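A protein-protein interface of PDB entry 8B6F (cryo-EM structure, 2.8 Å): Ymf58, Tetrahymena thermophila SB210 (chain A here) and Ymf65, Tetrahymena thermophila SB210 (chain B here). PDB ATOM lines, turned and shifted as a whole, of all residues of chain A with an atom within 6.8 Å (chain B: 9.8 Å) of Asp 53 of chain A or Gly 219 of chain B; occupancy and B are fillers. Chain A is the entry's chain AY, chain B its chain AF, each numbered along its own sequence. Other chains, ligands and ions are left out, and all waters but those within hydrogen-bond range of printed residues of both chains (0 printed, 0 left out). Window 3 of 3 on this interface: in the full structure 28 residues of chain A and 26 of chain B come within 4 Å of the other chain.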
ATOM      1  N   SER A  44      -9.645   3.940  28.712  1.00  0.00           N
ATOM      2  CA  SER A  44     -10.963   4.563  28.674  1.00  0.00           C
ATOM      3  C   SER A  44     -11.866   4.006  29.765  1.00  0.00           C
ATOM      4  O   SER A  44     -12.601   4.757  30.416  1.00  0.00           O
ATOM      5  CB  SER A  44     -11.596   4.364  27.297  1.00  0.00           C
ATOM      6  OG  SER A  44     -11.725   2.988  26.989  1.00  0.00           O
ATOM      7  N   PHE A  47     -10.781   5.572  33.150  1.00  0.00           N
ATOM      8  CA  PHE A  47     -11.240   6.946  33.321  1.00  0.00           C
ATOM      9  C   PHE A  47     -12.753   7.008  33.480  1.00  0.00           C
ATOM     10  O   PHE A  47     -13.268   7.823  34.254  1.00  0.00           O
ATOM     11  CB  PHE A  47     -10.789   7.809  32.143  1.00  0.00           C
ATOM     12  CG  PHE A  47      -9.383   8.329  32.271  1.00  0.00           C
ATOM     13  CD1 PHE A  47      -8.485   7.751  33.153  1.00  0.00           C
ATOM     14  CD2 PHE A  47      -8.967   9.411  31.515  1.00  0.00           C
ATOM     15  CE1 PHE A  47      -7.200   8.236  33.270  1.00  0.00           C
ATOM     16  CE2 PHE A  47      -7.683   9.899  31.629  1.00  0.00           C
ATOM     17  CZ  PHE A  47      -6.798   9.311  32.506  1.00  0.00           C
ATOM     18  N   GLY A  48     -13.483   6.159  32.758  1.00  0.00           N
ATOM     19  CA  GLY A  48     -14.926   6.120  32.925  1.00  0.00           C
ATOM     20  C   GLY A  48     -15.337   5.726  34.328  1.00  0.00           C
ATOM     21  O   GLY A  48     -16.258   6.309  34.904  1.00  0.00           O
ATOM     22  N   ALA A  49     -14.666   4.725  34.899  1.00  0.00           N
ATOM     23  CA  ALA A  49     -14.947   4.346  36.278  1.00  0.00           C
ATOM     24  C   ALA A  49     -14.615   5.481  37.237  1.00  0.00           C
ATOM     25  O   ALA A  49     -15.358   5.736  38.191  1.00  0.00           O
ATOM     26  CB  ALA A  49     -14.159   3.089  36.645  1.00  0.00           C
ATOM     27  N   ILE A  50     -13.493   6.166  37.007  1.00  0.00           N
ATOM     28  CA  ILE A  50     -13.062   7.223  37.916  1.00  0.00           C
ATOM     29  C   ILE A  50     -14.057   8.376  37.908  1.00  0.00           C
ATOM     30  O   ILE A  50     -14.449   8.889  38.961  1.00  0.00           O
ATOM     31  CB  ILE A  50     -11.648   7.700  37.536  1.00  0.00           C
ATOM     32  CG1 ILE A  50     -10.623   6.623  37.886  1.00  0.00           C
ATOM     33  CG2 ILE A  50     -11.302   9.008  38.240  1.00  0.00           C
ATOM     34  CD1 ILE A  50      -9.252   6.883  37.322  1.00  0.00           C
ATOM     35  N   TYR A  51     -14.475   8.807  36.718  1.00  0.00           N
ATOM     36  CA  TYR A  51     -15.279  10.013  36.574  1.00  0.00           C
ATOM     37  C   TYR A  51     -16.767   9.727  36.427  1.00  0.00           C
ATOM     38  O   TYR A  51     -17.543  10.658  36.197  1.00  0.00           O
ATOM     39  CB  TYR A  51     -14.787  10.823  35.374  1.00  0.00           C
ATOM     40  CG  TYR A  51     -13.389  11.368  35.543  1.00  0.00           C
ATOM     41  CD1 TYR A  51     -13.142  12.451  36.373  1.00  0.00           C
ATOM     42  CD2 TYR A  51     -12.317  10.802  34.865  1.00  0.00           C
ATOM     43  CE1 TYR A  51     -11.866  12.953  36.529  1.00  0.00           C
ATOM     44  CE2 TYR A  51     -11.037  11.297  35.016  1.00  0.00           C
ATOM     45  CZ  TYR A  51     -10.819  12.372  35.849  1.00  0.00           C
ATOM     46  OH  TYR A  51      -9.547  12.871  36.001  1.00  0.00           O
ATOM     47  N   CYS A  52     -17.186   8.470  36.559  1.00  0.00           N
ATOM     48  CA  CYS A  52     -18.599   8.109  36.461  1.00  0.00           C
ATOM     49  C   CYS A  52     -19.178   8.520  35.109  1.00  0.00           C
ATOM     50  O   CYS A  52     -20.306   9.006  35.019  1.00  0.00           O
ATOM     51  CB  CYS A  52     -19.397   8.739  37.604  1.00  0.00           C
ATOM     52  SG  CYS A  52     -21.035   8.041  37.852  1.00  0.00           S
ATOM     53  N   ASP A  53     -18.406   8.317  34.046  1.00  0.00           N
ATOM     54  CA  ASP A  53     -18.764   8.773  32.705  1.00  0.00           C
ATOM     55  C   ASP A  53     -19.206   7.578  31.868  1.00  0.00           C
ATOM     56  O   ASP A  53     -18.378   6.757  31.464  1.00  0.00           O
ATOM     57  CB  ASP A  53     -17.589   9.497  32.055  1.00  0.00           C
ATOM     58  CG  ASP A  53     -17.989  10.250  30.802  1.00  0.00           C
ATOM     59  OD1 ASP A  53     -19.158  10.129  30.381  1.00  0.00           O
ATOM     60  OD2 ASP A  53     -17.137  10.969  30.240  1.00  0.00           O
ATOM     61  N   ILE A  54     -20.512   7.485  31.603  1.00  0.00           N
ATOM     62  CA  ILE A  54     -21.028   6.384  30.793  1.00  0.00           C
ATOM     63  C   ILE A  54     -20.483   6.459  29.374  1.00  0.00           C
ATOM     64  O   ILE A  54     -20.335   5.430  28.703  1.00  0.00           O
ATOM     65  CB  ILE A  54     -22.569   6.362  30.800  1.00  0.00           C
ATOM     66  CG1 ILE A  54     -23.134   7.648  30.208  1.00  0.00           C
ATOM     67  CG2 ILE A  54     -23.082   6.190  32.217  1.00  0.00           C
ATOM     68  CD1 ILE A  54     -24.602   7.565  29.854  1.00  0.00           C
ATOM     69  N   THR A  55     -20.186   7.664  28.887  1.00  0.00           N
ATOM     70  CA  THR A  55     -19.593   7.798  27.560  1.00  0.00           C
ATOM     71  C   THR A  55     -18.215   7.150  27.517  1.00  0.00           C
ATOM     72  O   THR A  55     -17.886   6.429  26.569  1.00  0.00           O
ATOM     73  CB  THR A  55     -19.506   9.273  27.168  1.00  0.00           C
ATOM     74  OG1 THR A  55     -20.806   9.873  27.245  1.00  0.00           O
ATOM     75  CG2 THR A  55     -18.976   9.419  25.748  1.00  0.00           C
ATOM     76  N   LEU A  56     -17.388   7.404  28.532  1.00  0.00           N
ATOM     77  CA  LEU A  56     -16.072   6.772  28.584  1.00  0.00           C
ATOM     78  C   LEU A  56     -16.187   5.258  28.705  1.00  0.00           C
ATOM     79  O   LEU A  56     -15.432   4.519  28.065  1.00  0.00           O
ATOM     80  CB  LEU A  56     -15.261   7.347  29.744  1.00  0.00           C
ATOM     81  CG  LEU A  56     -14.721   8.766  29.546  1.00  0.00           C
ATOM     82  CD1 LEU A  56     -14.062   9.268  30.812  1.00  0.00           C
ATOM     83  CD2 LEU A  56     -13.739   8.818  28.391  1.00  0.00           C
ATOM     84  N   LEU A  57     -17.127   4.774  29.519  1.00  0.00           N
ATOM     85  CA  LEU A  57     -17.332   3.334  29.631  1.00  0.00           C
ATOM     86  C   LEU A  57     -17.768   2.744  28.299  1.00  0.00           C
ATOM     87  O   LEU A  57     -17.313   1.663  27.908  1.00  0.00           O
ATOM     88  CB  LEU A  57     -18.360   3.001  30.709  1.00  0.00           C
ATOM     89  CG  LEU A  57     -17.923   3.086  32.171  1.00  0.00           C
ATOM     90  CD1 LEU A  57     -19.027   2.526  33.032  1.00  0.00           C
ATOM     91  CD2 LEU A  57     -16.618   2.356  32.439  1.00  0.00           C
ATOM     92  N   SER A  58     -18.651   3.439  27.591  1.00  0.00           N
ATOM     93  CA  SER A  58     -19.193   2.920  26.348  1.00  0.00           C
ATOM     94  C   SER A  58     -18.210   3.012  25.196  1.00  0.00           C
ATOM     95  O   SER A  58     -18.403   2.338  24.178  1.00  0.00           O
ATOM     96  CB  SER A  58     -20.408   3.748  25.971  1.00  0.00           C
ATOM     97  OG  SER A  58     -19.943   5.076  25.766  1.00  0.00           O
ATOM     98  N   HIS B  88     -25.170  16.589  20.046  1.00  0.00           N
ATOM     99  CA  HIS B  88     -24.055  16.030  19.297  1.00  0.00           C
ATOM    100  C   HIS B  88     -23.841  16.715  17.958  1.00  0.00           C
ATOM    101  O   HIS B  88     -22.763  16.574  17.374  1.00  0.00           O
ATOM    102  CB  HIS B  88     -24.271  14.532  19.071  1.00  0.00           C
ATOM    103  CG  HIS B  88     -23.937  13.692  20.265  1.00  0.00           C
ATOM    104  ND1 HIS B  88     -24.367  14.002  21.537  1.00  0.00           N
ATOM    105  CD2 HIS B  88     -23.207  12.560  20.381  1.00  0.00           C
ATOM    106  CE1 HIS B  88     -23.920  13.094  22.384  1.00  0.00           C
ATOM    107  NE2 HIS B  88     -23.213  12.206  21.708  1.00  0.00           N
ATOM    108  N   PHE B 148     -16.132  13.887  19.998  1.00  0.00           N
ATOM    109  CA  PHE B 148     -16.496  12.481  19.859  1.00  0.00           C
ATOM    110  C   PHE B 148     -17.171  12.219  18.520  1.00  0.00           C
ATOM    111  O   PHE B 148     -16.746  11.343  17.758  1.00  0.00           O
ATOM    112  CB  PHE B 148     -17.416  12.077  21.012  1.00  0.00           C
ATOM    113  CG  PHE B 148     -17.472  10.602  21.263  1.00  0.00           C
ATOM    114  CD1 PHE B 148     -16.342   9.908  21.654  1.00  0.00           C
ATOM    115  CD2 PHE B 148     -18.669   9.915  21.150  1.00  0.00           C
ATOM    116  CE1 PHE B 148     -16.396   8.552  21.899  1.00  0.00           C
ATOM    117  CE2 PHE B 148     -18.731   8.558  21.393  1.00  0.00           C
ATOM    118  CZ  PHE B 148     -17.592   7.875  21.769  1.00  0.00           C
ATOM    119  N   ILE B 211      -9.314  12.471  23.109  1.00  0.00           N
ATOM    120  CA  ILE B 211     -10.714  12.507  23.521  1.00  0.00           C
ATOM    121  C   ILE B 211     -10.860  12.022  24.954  1.00  0.00           C
ATOM    122  O   ILE B 211     -11.599  12.610  25.751  1.00  0.00           O
ATOM    123  CB  ILE B 211     -11.579  11.676  22.553  1.00  0.00           C
ATOM    124  CG1 ILE B 211     -11.733  12.408  21.220  1.00  0.00           C
ATOM    125  CG2 ILE B 211     -12.955  11.396  23.155  1.00  0.00           C
ATOM    126  CD1 ILE B 211     -12.333  11.564  20.120  1.00  0.00           C
ATOM    127  N   ILE B 212     -10.171  10.937  25.304  1.00  0.00           N
ATOM    128  CA  ILE B 212     -10.259  10.423  26.667  1.00  0.00           C
ATOM    129  C   ILE B 212      -9.769  11.465  27.661  1.00  0.00           C
ATOM    130  O   ILE B 212     -10.398  11.691  28.701  1.00  0.00           O
ATOM    131  CB  ILE B 212      -9.467   9.107  26.784  1.00  0.00           C
ATOM    132  CG1 ILE B 212     -10.156   8.008  25.975  1.00  0.00           C
ATOM    133  CG2 ILE B 212      -9.318   8.689  28.245  1.00  0.00           C
ATOM    134  CD1 ILE B 212      -9.314   6.771  25.785  1.00  0.00           C
ATOM    135  N   TYR B 213      -8.642  12.114  27.368  1.00  0.00           N
ATOM    136  CA  TYR B 213      -8.101  13.072  28.323  1.00  0.00           C
ATOM    137  C   TYR B 213      -8.898  14.369  28.349  1.00  0.00           C
ATOM    138  O   TYR B 213      -8.941  15.044  29.382  1.00  0.00           O
ATOM    139  CB  TYR B 213      -6.630  13.345  28.027  1.00  0.00           C
ATOM    140  CG  TYR B 213      -5.740  12.624  29.000  1.00  0.00           C
ATOM    141  CD1 TYR B 213      -5.521  13.131  30.272  1.00  0.00           C
ATOM    142  CD2 TYR B 213      -5.146  11.419  28.661  1.00  0.00           C
ATOM    143  CE1 TYR B 213      -4.725  12.464  31.174  1.00  0.00           C
ATOM    144  CE2 TYR B 213      -4.348  10.745  29.555  1.00  0.00           C
ATOM    145  CZ  TYR B 213      -4.139  11.274  30.808  1.00  0.00           C
ATOM    146  OH  TYR B 213      -3.340  10.599  31.694  1.00  0.00           O
ATOM    147  N   LEU B 214      -9.529  14.739  27.234  1.00  0.00           N
ATOM    148  CA  LEU B 214     -10.438  15.880  27.261  1.00  0.00           C
ATOM    149  C   LEU B 214     -11.666  15.578  28.108  1.00  0.00           C
ATOM    150  O   LEU B 214     -12.171  16.457  28.814  1.00  0.00           O
ATOM    151  CB  LEU B 214     -10.843  16.277  25.842  1.00  0.00           C
ATOM    152  CG  LEU B 214      -9.842  17.138  25.069  1.00  0.00           C
ATOM    153  CD1 LEU B 214     -10.265  17.274  23.619  1.00  0.00           C
ATOM    154  CD2 LEU B 214      -9.700  18.513  25.701  1.00  0.00           C
ATOM    155  N   PHE B 215     -12.169  14.344  28.043  1.00  0.00           N
ATOM    156  CA  PHE B 215     -13.253  13.951  28.935  1.00  0.00           C
ATOM    157  C   PHE B 215     -12.811  14.009  30.391  1.00  0.00           C
ATOM    158  O   PHE B 215     -13.575  14.437  31.263  1.00  0.00           O
ATOM    159  CB  PHE B 215     -13.743  12.545  28.583  1.00  0.00           C
ATOM    160  CG  PHE B 215     -14.949  12.529  27.691  1.00  0.00           C
ATOM    161  CD1 PHE B 215     -16.200  12.843  28.193  1.00  0.00           C
ATOM    162  CD2 PHE B 215     -14.835  12.192  26.353  1.00  0.00           C
ATOM    163  CE1 PHE B 215     -17.314  12.827  27.378  1.00  0.00           C
ATOM    164  CE2 PHE B 215     -15.946  12.174  25.532  1.00  0.00           C
ATOM    165  CZ  PHE B 215     -17.186  12.492  26.045  1.00  0.00           C
ATOM    166  N   SER B 216     -11.587  13.565  30.679  1.00  0.00           N
ATOM    167  CA  SER B 216     -11.085  13.634  32.048  1.00  0.00           C
ATOM    168  C   SER B 216     -10.990  15.078  32.520  1.00  0.00           C
ATOM    169  O   SER B 216     -11.408  15.411  33.634  1.00  0.00           O
ATOM    170  CB  SER B 216      -9.722  12.948  32.144  1.00  0.00           C
ATOM    171  OG  SER B 216      -8.692  13.791  31.659  1.00  0.00           O
ATOM    172  N   LEU B 217     -10.447  15.954  31.673  1.00  0.00           N
ATOM    173  CA  LEU B 217     -10.263  17.350  32.061  1.00  0.00           C
ATOM    174  C   LEU B 217     -11.604  18.050  32.244  1.00  0.00           C
ATOM    175  O   LEU B 217     -11.841  18.701  33.267  1.00  0.00           O
ATOM    176  CB  LEU B 217      -9.414  18.071  31.013  1.00  0.00           C
ATOM    177  CG  LEU B 217      -9.191  19.570  31.231  1.00  0.00           C
ATOM    178  CD1 LEU B 217      -8.521  19.835  32.568  1.00  0.00           C
ATOM    179  CD2 LEU B 217      -8.367  20.148  30.096  1.00  0.00           C
ATOM    180  N   THR B 218     -12.488  17.931  31.259  1.00  0.00           N
ATOM    181  CA  THR B 218     -13.826  18.500  31.321  1.00  0.00           C
ATOM    182  C   THR B 218     -14.843  17.376  31.201  1.00  0.00           C
ATOM    183  O   THR B 218     -14.708  16.496  30.347  1.00  0.00           O
ATOM    184  CB  THR B 218     -14.052  19.517  30.203  1.00  0.00           C
ATOM    185  OG1 THR B 218     -14.189  18.832  28.953  1.00  0.00           O
ATOM    186  CG2 THR B 218     -12.861  20.456  30.092  1.00  0.00           C
ATOM    187  N   GLY B 219     -15.868  17.414  32.045  1.00  0.00           N
ATOM    188  CA  GLY B 219     -16.840  16.339  32.100  1.00  0.00           C
ATOM    189  C   GLY B 219     -17.422  15.946  30.757  1.00  0.00           C
ATOM    190  O   GLY B 219     -17.935  14.833  30.607  1.00  0.00           O
ATOM    191  N   SER B 220     -17.358  16.840  29.778  1.00  0.00           N
ATOM    192  CA  SER B 220     -17.886  16.597  28.443  1.00  0.00           C
ATOM    193  C   SER B 220     -16.778  16.777  27.414  1.00  0.00           C
ATOM    194  O   SER B 220     -15.629  17.077  27.745  1.00  0.00           O
ATOM    195  CB  SER B 220     -19.059  17.532  28.134  1.00  0.00           C
ATOM    196  OG  SER B 220     -18.648  18.885  28.127  1.00  0.00           O
ATOM    197  N   THR B 221     -17.143  16.582  26.147  1.00  0.00           N
ATOM    198  CA  THR B 221     -16.248  16.838  25.028  1.00  0.00           C
ATOM    199  C   THR B 221     -16.868  17.797  24.018  1.00  0.00           C
ATOM    200  O   THR B 221     -16.374  17.895  22.888  1.00  0.00           O
ATOM    201  CB  THR B 221     -15.847  15.521  24.350  1.00  0.00           C
ATOM    202  OG1 THR B 221     -14.776  15.755  23.427  1.00  0.00           O
ATOM    203  CG2 THR B 221     -17.013  14.906  23.613  1.00  0.00           C
ATOM    204  N   GLU B 222     -17.940  18.490  24.389  1.00  0.00           N
ATOM    205  CA  GLU B 222     -18.543  19.489  23.521  1.00  0.00           C
ATOM    206  C   GLU B 222     -17.634  20.705  23.398  1.00  0.00           C
ATOM    207  O   GLU B 222     -16.945  21.093  24.344  1.00  0.00           O
ATOM    208  CB  GLU B 222     -19.905  19.909  24.073  1.00  0.00           C
ATOM    209  CG  GLU B 222     -20.632  20.938  23.233  1.00  0.00           C
ATOM    210  CD  GLU B 222     -21.992  21.275  23.802  1.00  0.00           C
ATOM    211  OE1 GLU B 222     -22.420  20.592  24.755  1.00  0.00           O
ATOM    212  OE2 GLU B 222     -22.633  22.224  23.302  1.00  0.00           O
ATOM    213  N   ILE B 225     -18.542  23.694  25.857  1.00  0.00           N
ATOM    214  CA  ILE B 225     -18.211  23.382  27.243  1.00  0.00           C
ATOM    215  C   ILE B 225     -16.701  23.338  27.435  1.00  0.00           C
ATOM    216  O   ILE B 225     -16.180  23.808  28.452  1.00  0.00           O
ATOM    217  CB  ILE B 225     -18.881  22.065  27.675  1.00  0.00           C
ATOM    218  CG1 ILE B 225     -20.407  22.182  27.602  1.00  0.00           C
ATOM    219  CG2 ILE B 225     -18.446  21.687  29.089  1.00  0.00           C
ATOM    220  CD1 ILE B 225     -21.008  23.240  28.509  1.00  0.00           C
ATOM    221  N   ILE B 226     -15.972  22.765  26.475  1.00  0.00           N
ATOM    222  CA  ILE B 226     -14.517  22.710  26.590  1.00  0.00           C
ATOM    223  C   ILE B 226     -13.942  24.118  26.674  1.00  0.00           C
ATOM    224  O   ILE B 226     -13.131  24.424  27.554  1.00  0.00           O
ATOM    225  CB  ILE B 226     -13.914  21.927  25.408  1.00  0.00           C
ATOM    226  CG1 ILE B 226     -14.198  20.431  25.559  1.00  0.00           C
ATOM    227  CG2 ILE B 226     -12.406  22.171  25.303  1.00  0.00           C
ATOM    228  CD1 ILE B 226     -13.847  19.620  24.329  1.00  0.00           C
ATOM    229  N   ILE B 229     -14.894  25.833  30.028  1.00  0.00           N
ATOM    230  CA  ILE B 229     -14.175  25.281  31.171  1.00  0.00           C
ATOM    231  C   ILE B 229     -12.712  25.709  31.153  1.00  0.00           C
ATOM    232  O   ILE B 229     -12.135  26.032  32.197  1.00  0.00           O
ATOM    233  CB  ILE B 229     -14.316  23.749  31.201  1.00  0.00           C
ATOM    234  CG1 ILE B 229     -15.764  23.333  31.484  1.00  0.00           C
ATOM    235  CG2 ILE B 229     -13.379  23.164  32.244  1.00  0.00           C
ATOM    236  CD1 ILE B 229     -16.265  23.660  32.873  1.00  0.00           C
ATOM    237  N   VAL B 230     -12.085  25.714  29.975  1.00  0.00           N
ATOM    238  CA  VAL B 230     -10.683  26.119  29.885  1.00  0.00           C
ATOM    239  C   VAL B 230     -10.522  27.585  30.264  1.00  0.00           C
ATOM    240  O   VAL B 230      -9.589  27.952  30.989  1.00  0.00           O
ATOM    241  CB  VAL B 230     -10.134  25.838  28.473  1.00  0.00           C
ATOM    242  CG1 VAL B 230      -8.759  26.469  28.287  1.00  0.00           C
ATOM    243  CG2 VAL B 230     -10.051  24.344  28.224  1.00  0.00           C
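The backbone carbonyl oxygen (O) of Gly 48 of chain A is in hydrogen-bond range of the backbone NH (N) of Asp 53 of chain A. The backbone NH (N) of Thr 55 of chain A is in hydrogen-bond range of the side-chain carboxylate (OD1) of Asp 53 of chain A, 3.1 Å away. The backbone carbonyl oxygen (O) of Thr 55 of chain A lies within hydrogen-bond range of the side-chain hydroxyl (OG) of Ser 58 of chain A, 2.6 Å away. OG of Ser 216 of chain B lies within hydrogen-bond range of O of Tyr 213 of chain B (2.6 Å).
Among the printed residues, merely in contact across the chains: Ser 44 of chain A with Ile 212 of chain B, Phe 47 of chain A with Ile 212 of chain B, Phe 47 of chain A with Tyr 213 of chain B, Phe 47 of chain A with Ser 216 of chain B, Tyr 51 of chain A with Ser 216 of chain B, Asp 53 of chain A with Phe 215 of chain B, Asp 53 of chain A with Gly 219 of chain B, Thr 55 of chain A with Phe 215 of chain B and Leu 56 of chain A with Phe 215 of chain B.
Of chain B, only Phe 215 and Gly 219 come within 4 Å of Asp 53 of chain A. Thr 55 of chain A touches just one residue of chain B: Phe 215. Leu 56 of chain A touches just one residue of chain B: Phe 215 (3.7 Å). Of the printed residues of chain A, Ile 212 of chain B touches Ser 44 and Phe 47. Of the printed residues of chain B, Ser 44 of chain A touches Ile 212. The nearest residue of chain B that does not touch Asp 53 of chain A is Ser 220 of chain B (5.9 Å). The nearest residue of chain A that does not touch Gly 219 of chain B is Thr 55 of chain A (6.6 Å). The nearest printed residue of chain B that does not touch Tyr 51 of chain A is Phe 215 of chain B (5.3 Å).
Of the 18 printed residues of chain B, 5 touch a printed residue of chain A. Printed residues of chain B that touch a printed residue of chain A: Ile 212, Tyr 213, Phe 215, Ser 216 and Gly 219. Hydrophobic or aromatic side chains of chain B within 4 Å of the printed part of chain A: Ile 212, Tyr 213 and Phe 215. Of the 13 printed residues of chain A, 6 touch a printed residue of chain B. Hydrophobic or aromatic side chains of chain A within 4 Å of the printed part of chain B: Phe 47, Tyr 51 and Leu 56. Along chain A the printed residues that touch a printed residue of chain B span positions 44 to 56.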
